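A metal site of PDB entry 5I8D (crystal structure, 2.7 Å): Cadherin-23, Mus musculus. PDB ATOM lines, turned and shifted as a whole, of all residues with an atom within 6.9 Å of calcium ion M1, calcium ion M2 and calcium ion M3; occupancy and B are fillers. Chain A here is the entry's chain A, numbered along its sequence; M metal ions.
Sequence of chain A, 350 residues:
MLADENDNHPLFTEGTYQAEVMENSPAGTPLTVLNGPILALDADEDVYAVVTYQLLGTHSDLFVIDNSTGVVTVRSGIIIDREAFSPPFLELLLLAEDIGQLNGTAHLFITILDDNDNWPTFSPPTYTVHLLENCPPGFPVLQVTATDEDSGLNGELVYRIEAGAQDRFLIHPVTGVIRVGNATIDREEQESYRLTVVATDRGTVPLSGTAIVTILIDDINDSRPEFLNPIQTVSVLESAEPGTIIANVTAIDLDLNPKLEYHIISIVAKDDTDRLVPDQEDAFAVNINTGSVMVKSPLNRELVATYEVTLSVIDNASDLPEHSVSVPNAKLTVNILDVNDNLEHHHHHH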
ATOM      1  N   GLU A 133      -4.707   4.381  -0.017  1.00  0.00           N
ATOM      2  CA  GLU A 133      -5.087   5.050   1.226  1.00  0.00           C
ATOM      3  C   GLU A 133      -4.899   6.586   1.206  1.00  0.00           C
ATOM      4  O   GLU A 133      -4.111   7.106   0.418  1.00  0.00           O
ATOM      5  CB  GLU A 133      -4.247   4.376   2.332  1.00  0.00           C
ATOM      6  CG  GLU A 133      -4.241   5.012   3.700  1.00  0.00           C
ATOM      7  CD  GLU A 133      -3.327   4.265   4.665  1.00  0.00           C
ATOM      8  OE1 GLU A 133      -3.359   4.661   5.855  1.00  0.00           O
ATOM      9  OE2 GLU A 133      -2.572   3.328   4.248  1.00  0.00           O
ATOM     10  N   ASN A 134      -5.643   7.303   2.080  1.00  0.00           N
ATOM     11  CA  ASN A 134      -5.550   8.804   2.171  1.00  0.00           C
ATOM     12  C   ASN A 134      -5.793   9.545   0.852  1.00  0.00           C
ATOM     13  O   ASN A 134      -4.957  10.289   0.375  1.00  0.00           O
ATOM     14  CB  ASN A 134      -4.179   9.272   2.694  1.00  0.00           C
ATOM     15  CG  ASN A 134      -3.848   8.706   4.032  1.00  0.00           C
ATOM     16  OD1 ASN A 134      -4.649   8.765   4.945  1.00  0.00           O
ATOM     17  ND2 ASN A 134      -2.649   8.159   4.166  1.00  0.00           N
ATOM     18  N   ILE A 185     -10.130   7.742   4.273  1.00  0.00           N
ATOM     19  CA  ILE A 185      -9.912   6.341   3.851  1.00  0.00           C
ATOM     20  C   ILE A 185      -8.584   5.854   4.397  1.00  0.00           C
ATOM     21  O   ILE A 185      -7.513   6.081   3.783  1.00  0.00           O
ATOM     22  CB  ILE A 185      -9.923   6.204   2.312  1.00  0.00           C
ATOM     23  CG1 ILE A 185     -11.280   6.620   1.743  1.00  0.00           C
ATOM     24  CG2 ILE A 185      -9.541   4.789   1.857  1.00  0.00           C
ATOM     25  CD1 ILE A 185     -12.476   5.850   2.274  1.00  0.00           C
ATOM     26  N   ASP A 186      -8.672   5.192   5.551  1.00  0.00           N
ATOM     27  CA  ASP A 186      -7.523   4.654   6.293  1.00  0.00           C
ATOM     28  C   ASP A 186      -7.460   3.128   6.260  1.00  0.00           C
ATOM     29  O   ASP A 186      -8.262   2.441   6.917  1.00  0.00           O
ATOM     30  CB  ASP A 186      -7.592   5.121   7.743  1.00  0.00           C
ATOM     31  CG  ASP A 186      -6.348   4.762   8.548  1.00  0.00           C
ATOM     32  OD1 ASP A 186      -5.326   4.379   7.948  1.00  0.00           O
ATOM     33  OD2 ASP A 186      -6.387   4.870   9.787  1.00  0.00           O
ATOM     34  N   ARG A 187      -6.486   2.604   5.532  1.00  0.00           N
ATOM     35  CA  ARG A 187      -6.215   1.155   5.493  1.00  0.00           C
ATOM     36  C   ARG A 187      -6.024   0.504   6.864  1.00  0.00           C
ATOM     37  O   ARG A 187      -6.276  -0.707   7.007  1.00  0.00           O
ATOM     38  CB  ARG A 187      -4.975   0.855   4.659  1.00  0.00           C
ATOM     39  CG  ARG A 187      -4.992  -0.555   4.084  1.00  0.00           C
ATOM     40  CD  ARG A 187      -3.608  -1.046   3.763  1.00  0.00           C
ATOM     41  NE  ARG A 187      -2.836  -1.250   4.989  1.00  0.00           N
ATOM     42  CZ  ARG A 187      -2.827  -2.347   5.749  1.00  0.00           C
ATOM     43  NH1 ARG A 187      -3.557  -3.439   5.431  1.00  0.00           N
ATOM     44  NH2 ARG A 187      -2.074  -2.357   6.838  1.00  0.00           N
ATOM     45  N   GLU A 188      -5.560   1.279   7.842  1.00  0.00           N
ATOM     46  CA  GLU A 188      -5.420   0.806   9.229  1.00  0.00           C
ATOM     47  C   GLU A 188      -6.767   0.718   9.967  1.00  0.00           C
ATOM     48  O   GLU A 188      -6.888  -0.036  10.927  1.00  0.00           O
ATOM     49  CB  GLU A 188      -4.403   1.653  10.022  1.00  0.00           C
ATOM     50  CG  GLU A 188      -2.937   1.325   9.741  1.00  0.00           C
ATOM     51  CD  GLU A 188      -2.508   1.536   8.288  1.00  0.00           C
ATOM     52  OE1 GLU A 188      -2.142   0.541   7.597  1.00  0.00           O
ATOM     53  OE2 GLU A 188      -2.512   2.720   7.826  1.00  0.00           O
ATOM     54  N   GLU A 189      -7.754   1.492   9.511  1.00  0.00           N
ATOM     55  CA  GLU A 189      -9.153   1.401   9.996  1.00  0.00           C
ATOM     56  C   GLU A 189      -9.891   0.307   9.234  1.00  0.00           C
ATOM     57  O   GLU A 189     -10.556  -0.512   9.848  1.00  0.00           O
ATOM     58  CB  GLU A 189      -9.902   2.743   9.873  1.00  0.00           C
ATOM     59  CG  GLU A 189     -11.395   2.670  10.167  1.00  0.00           C
ATOM     60  CD  GLU A 189     -11.985   4.035  10.503  1.00  0.00           C
ATOM     61  OE1 GLU A 189     -12.604   4.150  11.587  1.00  0.00           O
ATOM     62  OE2 GLU A 189     -11.845   4.972   9.690  1.00  0.00           O
ATOM     63  N   ASP A 218      -5.049  -0.065  -0.673  1.00  0.00           N
ATOM     64  CA  ASP A 218      -3.586  -0.236  -0.737  1.00  0.00           C
ATOM     65  C   ASP A 218      -2.927   0.605   0.351  1.00  0.00           C
ATOM     66  O   ASP A 218      -3.512   1.570   0.845  1.00  0.00           O
ATOM     67  CB  ASP A 218      -3.039   0.065  -2.139  1.00  0.00           C
ATOM     68  CG  ASP A 218      -3.231  -1.102  -3.118  1.00  0.00           C
ATOM     69  OD1 ASP A 218      -3.895  -2.101  -2.743  1.00  0.00           O
ATOM     70  OD2 ASP A 218      -2.733  -1.028  -4.258  1.00  0.00           O
ATOM     71  N   ASP A 219      -1.721   0.213   0.738  1.00  0.00           N
ATOM     72  CA  ASP A 219      -1.043   0.764   1.907  1.00  0.00           C
ATOM     73  C   ASP A 219      -0.035   1.829   1.533  1.00  0.00           C
ATOM     74  O   ASP A 219       0.798   1.619   0.656  1.00  0.00           O
ATOM     75  CB  ASP A 219      -0.297  -0.343   2.648  1.00  0.00           C
ATOM     76  CG  ASP A 219       0.397   0.160   3.896  1.00  0.00           C
ATOM     77  OD1 ASP A 219      -0.304   0.735   4.760  1.00  0.00           O
ATOM     78  OD2 ASP A 219       1.622  -0.020   4.004  1.00  0.00           O
ATOM     79  N   ILE A 220      -0.113   2.969   2.228  1.00  0.00           N
ATOM     80  CA  ILE A 220       1.018   3.846   2.396  1.00  0.00           C
ATOM     81  C   ILE A 220       1.476   3.543   3.823  1.00  0.00           C
ATOM     82  O   ILE A 220       0.646   3.356   4.710  1.00  0.00           O
ATOM     83  CB  ILE A 220       0.605   5.337   2.298  1.00  0.00           C
ATOM     84  CG1 ILE A 220       0.084   5.671   0.897  1.00  0.00           C
ATOM     85  CG2 ILE A 220       1.789   6.255   2.614  1.00  0.00           C
ATOM     86  CD1 ILE A 220      -0.724   6.964   0.831  1.00  0.00           C
ATOM     87  N   ASN A 221       2.794   3.474   4.038  1.00  0.00           N
ATOM     88  CA  ASN A 221       3.353   3.347   5.403  1.00  0.00           C
ATOM     89  C   ASN A 221       3.299   4.702   6.133  1.00  0.00           C
ATOM     90  O   ASN A 221       4.265   5.493   6.095  1.00  0.00           O
ATOM     91  CB  ASN A 221       4.775   2.789   5.360  1.00  0.00           C
ATOM     92  CG  ASN A 221       5.280   2.422   6.752  1.00  0.00           C
ATOM     93  OD1 ASN A 221       5.163   3.195   7.709  1.00  0.00           O
ATOM     94  ND2 ASN A 221       5.850   1.220   6.876  1.00  0.00           N
ATOM     95  N   ASP A 222       2.179   4.933   6.818  1.00  0.00           N
ATOM     96  CA  ASP A 222       1.865   6.239   7.362  1.00  0.00           C
ATOM     97  C   ASP A 222       1.399   6.238   8.810  1.00  0.00           C
ATOM     98  O   ASP A 222       0.891   7.247   9.288  1.00  0.00           O
ATOM     99  CB  ASP A 222       0.770   6.862   6.499  1.00  0.00           C
ATOM    100  CG  ASP A 222      -0.558   6.167   6.641  1.00  0.00           C
ATOM    101  OD1 ASP A 222      -0.618   4.994   7.090  1.00  0.00           O
ATOM    102  OD2 ASP A 222      -1.568   6.802   6.296  1.00  0.00           O
ATOM    103  N   SER A 223       1.590   5.130   9.514  1.00  0.00           N
ATOM    104  CA  SER A 223       1.076   4.961  10.858  1.00  0.00           C
ATOM    105  C   SER A 223       2.271   4.827  11.796  1.00  0.00           C
ATOM    106  O   SER A 223       3.179   3.991  11.523  1.00  0.00           O
ATOM    107  CB  SER A 223       0.232   3.706  10.912  1.00  0.00           C
ATOM    108  OG  SER A 223      -0.588   3.724  12.050  1.00  0.00           O
ATOM    109  N   ARG A 224       2.327   5.650  12.852  1.00  0.00           N
ATOM    110  CA  ARG A 224       3.509   5.645  13.740  1.00  0.00           C
ATOM    111  C   ARG A 224       3.552   4.411  14.638  1.00  0.00           C
ATOM    112  O   ARG A 224       2.503   3.909  15.064  1.00  0.00           O
ATOM    113  CB  ARG A 224       3.644   6.956  14.562  1.00  0.00           C
ATOM    114  CG  ARG A 224       2.596   7.161  15.649  1.00  0.00           C
ATOM    115  CD  ARG A 224       2.923   8.337  16.574  1.00  0.00           C
ATOM    116  NE  ARG A 224       2.585   9.636  15.983  1.00  0.00           N
ATOM    117  CZ  ARG A 224       3.432  10.450  15.350  1.00  0.00           C
ATOM    118  NH1 ARG A 224       4.711  10.108  15.173  1.00  0.00           N
ATOM    119  NH2 ARG A 224       2.989  11.619  14.879  1.00  0.00           N
ATOM    120  N   PRO A 225       4.763   3.905  14.941  1.00  0.00           N
ATOM    121  CA  PRO A 225       4.876   2.798  15.847  1.00  0.00           C
ATOM    122  C   PRO A 225       4.480   3.215  17.248  1.00  0.00           C
ATOM    123  O   PRO A 225       4.792   4.338  17.698  1.00  0.00           O
ATOM    124  CB  PRO A 225       6.357   2.427  15.783  1.00  0.00           C
ATOM    125  CG  PRO A 225       7.045   3.642  15.344  1.00  0.00           C
ATOM    126  CD  PRO A 225       6.081   4.338  14.441  1.00  0.00           C
ATOM    127  N   ASP A 253       3.455  -1.723  14.997  1.00  0.00           N
ATOM    128  CA  ASP A 253       3.249  -0.807  13.884  1.00  0.00           C
ATOM    129  C   ASP A 253       2.228  -1.469  12.982  1.00  0.00           C
ATOM    130  O   ASP A 253       2.458  -2.578  12.523  1.00  0.00           O
ATOM    131  CB  ASP A 253       4.554  -0.573  13.139  1.00  0.00           C
ATOM    132  CG  ASP A 253       4.565   0.723  12.329  1.00  0.00           C
ATOM    133  OD1 ASP A 253       4.038   0.779  11.199  1.00  0.00           O
ATOM    134  OD2 ASP A 253       5.154   1.727  12.796  1.00  0.00           O
ATOM    135  N   LEU A 254       1.117  -0.791  12.734  1.00  0.00           N
ATOM    136  CA  LEU A 254      -0.006  -1.401  12.020  1.00  0.00           C
ATOM    137  C   LEU A 254       0.073  -1.328  10.497  1.00  0.00           C
ATOM    138  O   LEU A 254      -0.841  -1.781   9.806  1.00  0.00           O
ATOM    139  CB  LEU A 254      -1.307  -0.771  12.489  1.00  0.00           C
ATOM    140  CG  LEU A 254      -1.571  -0.875  13.988  1.00  0.00           C
ATOM    141  CD1 LEU A 254      -2.709   0.052  14.377  1.00  0.00           C
ATOM    142  CD2 LEU A 254      -1.865  -2.303  14.372  1.00  0.00           C
ATOM    143  N   ASP A 255       1.165  -0.779   9.965  1.00  0.00           N
ATOM    144  CA  ASP A 255       1.391  -0.755   8.517  1.00  0.00           C
ATOM    145  C   ASP A 255       1.805  -2.131   8.002  1.00  0.00           C
ATOM    146  O   ASP A 255       2.003  -3.073   8.777  1.00  0.00           O
ATOM    147  CB  ASP A 255       2.436   0.322   8.167  1.00  0.00           C
ATOM    148  CG  ASP A 255       1.886   1.735   8.267  1.00  0.00           C
ATOM    149  OD1 ASP A 255       0.827   1.998   7.656  1.00  0.00           O
ATOM    150  OD2 ASP A 255       2.516   2.592   8.943  1.00  0.00           O
ATOM    151  N   LEU A 256       1.944  -2.228   6.688  1.00  0.00           N
ATOM    152  CA  LEU A 256       2.074  -3.498   5.992  1.00  0.00           C
ATOM    153  C   LEU A 256       3.443  -4.163   6.130  1.00  0.00           C
ATOM    154  O   LEU A 256       3.514  -5.369   6.261  1.00  0.00           O
ATOM    155  CB  LEU A 256       1.693  -3.312   4.522  1.00  0.00           C
ATOM    156  CG  LEU A 256       1.086  -4.502   3.753  1.00  0.00           C
ATOM    157  CD1 LEU A 256      -0.127  -5.113   4.435  1.00  0.00           C
ATOM    158  CD2 LEU A 256       0.725  -4.027   2.352  1.00  0.00           C
ATOM    159  N   PRO A 258       6.605  -2.953   8.203  1.00  0.00           N
ATOM    160  CA  PRO A 258       7.403  -2.070   9.025  1.00  0.00           C
ATOM    161  C   PRO A 258       8.779  -2.626   9.328  1.00  0.00           C
ATOM    162  O   PRO A 258       8.923  -3.825   9.519  1.00  0.00           O
ATOM    163  CB  PRO A 258       6.593  -1.940  10.313  1.00  0.00           C
ATOM    164  CG  PRO A 258       5.747  -3.152  10.369  1.00  0.00           C
ATOM    165  CD  PRO A 258       5.608  -3.702   8.988  1.00  0.00           C
ATOM    166  N   LEU A 260      11.018  -1.741  12.205  1.00  0.00           N
ATOM    167  CA  LEU A 260      11.180  -1.075  13.483  1.00  0.00           C
ATOM    168  C   LEU A 260      12.593  -1.204  14.040  1.00  0.00           C
ATOM    169  O   LEU A 260      13.098  -2.308  14.186  1.00  0.00           O
ATOM    170  CB  LEU A 260      10.211  -1.677  14.508  1.00  0.00           C
ATOM    171  CG  LEU A 260       8.711  -1.697  14.209  1.00  0.00           C
ATOM    172  CD1 LEU A 260       7.926  -1.712  15.509  1.00  0.00           C
ATOM    173  CD2 LEU A 260       8.258  -0.511  13.404  1.00  0.00           C
ATOM    174  N   ASP A 315      10.238   3.554  12.542  1.00  0.00           N
ATOM    175  CA  ASP A 315       9.873   2.707  11.408  1.00  0.00           C
ATOM    176  C   ASP A 315      10.670   3.100  10.137  1.00  0.00           C
ATOM    177  O   ASP A 315      10.283   3.989   9.384  1.00  0.00           O
ATOM    178  CB  ASP A 315       8.362   2.806  11.169  1.00  0.00           C
ATOM    179  CG  ASP A 315       7.823   1.755  10.198  1.00  0.00           C
ATOM    180  OD1 ASP A 315       8.624   0.993   9.620  1.00  0.00           O
ATOM    181  OD2 ASP A 315       6.572   1.695  10.031  1.00  0.00           O
ATOM    182  N   ALA A 317      10.898   1.866   7.290  1.00  0.00           N
ATOM    183  CA  ALA A 317      10.100   1.786   6.072  1.00  0.00           C
ATOM    184  C   ALA A 317       9.130   2.949   5.896  1.00  0.00           C
ATOM    185  O   ALA A 317       8.489   3.041   4.861  1.00  0.00           O
ATOM    186  CB  ALA A 317       9.324   0.463   6.062  1.00  0.00           C
ATOM    187  N   SER A 318       9.024   3.837   6.884  1.00  0.00           N
ATOM    188  CA  SER A 318       8.021   4.923   6.872  1.00  0.00           C
ATOM    189  C   SER A 318       8.027   5.806   5.624  1.00  0.00           C
ATOM    190  O   SER A 318       9.083   6.239   5.178  1.00  0.00           O
ATOM    191  CB  SER A 318       8.221   5.823   8.091  1.00  0.00           C
ATOM    192  OG  SER A 318       7.343   6.988   8.016  1.00  0.00           O
ATOM    193  N   ASP A 319       6.818   6.085   5.095  1.00  0.00           N
ATOM    194  CA  ASP A 319       6.668   6.966   3.913  1.00  0.00           C
ATOM    195  C   ASP A 319       6.421   8.440   4.284  1.00  0.00           C
ATOM    196  O   ASP A 319       6.485   9.306   3.408  1.00  0.00           O
ATOM    197  CB  ASP A 319       5.552   6.448   3.006  1.00  0.00           C
ATOM    198  CG  ASP A 319       5.909   5.140   2.288  1.00  0.00           C
ATOM    199  OD1 ASP A 319       6.953   5.080   1.599  1.00  0.00           O
ATOM    200  OD2 ASP A 319       5.119   4.175   2.384  1.00  0.00           O
ATOM    201  N   HIS A 323       5.181  10.416  10.773  1.00  0.00           N
ATOM    202  CA  HIS A 323       4.600   9.215  11.382  1.00  0.00           C
ATOM    203  C   HIS A 323       5.600   8.044  11.381  1.00  0.00           C
ATOM    204  O   HIS A 323       5.246   6.871  11.082  1.00  0.00           O
ATOM    205  CB  HIS A 323       3.283   8.853  10.679  1.00  0.00           C
ATOM    206  CG  HIS A 323       2.232   9.921  10.773  1.00  0.00           C
ATOM    207  ND1 HIS A 323       1.175   9.998   9.885  1.00  0.00           N
ATOM    208  CD2 HIS A 323       2.067  10.947  11.638  1.00  0.00           C
ATOM    209  CE1 HIS A 323       0.417  11.036  10.211  1.00  0.00           C
ATOM    210  NE2 HIS A 323       0.931  11.619  11.269  1.00  0.00           N
ATOM    211  N   SER A 324       6.860   8.367  11.705  1.00  0.00           N
ATOM    212  CA  SER A 324       7.971   7.404  11.691  1.00  0.00           C
ATOM    213  C   SER A 324       8.515   7.080  13.066  1.00  0.00           C
ATOM    214  O   SER A 324       9.090   6.019  13.237  1.00  0.00           O
ATOM    215  CB  SER A 324       9.118   7.929  10.808  1.00  0.00           C
ATOM    216  OG  SER A 324       9.483   9.255  11.135  1.00  0.00           O
HETATM  217 CA    CA M   1      -0.936   2.496   6.096  1.00  0.00          CA
HETATM  218 CA    CA M   2      -3.161   5.103   7.690  1.00  0.00          CA
HETATM  219 CA    CA M   3       4.673   2.868  10.275  1.00  0.00          CA
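O of Asp 222 is in hydrogen-bond range of ND1 of His 323, 2.8 Å away. The backbone carbonyl oxygen of Asp 218 sits at hydrogen-bond distance from the backbone NH of Glu 133, 3.2 Å away. The side-chain carboxylate (OE1) of Glu 188 lies close to the guanidinium group (NH2) of Arg 187 (3.0 Å). The side-chain carboxylate (OD1) of Asp 315 sits close to the backbone NH (N) of Ala 317 (3.4 Å). The backbone NH of Asp 315 lies within hydrogen-bond range of the backbone carbonyl oxygen of Ser 324 (2.8 Å). OD1 of Asp 219 sits close to NE of Arg 187 (3.2 Å). The side-chain carboxylate (OD2) of Asp 222 lies close to the side-chain amide nitrogen (ND2) of Asn 134 (2.7 Å). The backbone NH (N) of Asp 319 lies within hydrogen-bond range of the backbone carbonyl oxygen (O) of Asn 221 (2.8 Å).
Within 4 Å of calcium ion M1: Glu 133, Glu 188, Asp 219, Ile 220, Asp 222 and Asp 255.
Four residues have an atom within 4 Å of calcium ion M2: Glu 133, Asp 186, Glu 188 and Asp 222. The nearest printed residue that does not touch calcium ion M2 is Arg 187 (4.7 Å).
Within 4 Å of calcium ion M3: Asn 221, Ser 223, Asp 253, Asp 255 and Asp 315.
O of Ile 220 binds calcium ion M1, 2.3 Å away. OD1 of Asp 219 is bound to calcium ion M1, at 2.3 Å. The side-chain carboxylate (OE2) of Glu 188 binds calcium ion M1 (2.4 Å). OD1 of Asp 255 binds calcium ion M1 (2.4 Å). OE2 of Glu 133 is bound to calcium ion M1, 2.6 Å away. Calcium ion M1 is bound by OD1 of Asp 222 (2.7 Å). Calcium ion M1 is bound by the side-chain carboxylate (OE1) of Glu 188. Calcium ion M1 has seven donor atoms within binding distance.
Calcium ion M2 is bound by the side-chain carboxylate (OE1) of Glu 133 (1.9 Å), the side-chain carboxylate (OD1) of Asp 186 (2.3 Å), the side-chain carboxylate (OE2) of Glu 188 (2.5 Å), the side-chain carboxylate (OD1) of Asp 222 (2.6 Å) and the side-chain carboxylate (OD2) of Asp 222 (2.7 Å).
Calcium ion M3 is bound by OD2 of Asp 315 (2.2 Å), O of Ser 223 (2.2 Å), OD1 of Asp 253 (2.4 Å), OD2 of Asp 255 (2.6 Å), OD1 of Asn 221 (2.6 Å) and OD2 of Asp 253 (2.8 Å). Calcium ion M3 has six donor atoms within binding distance.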
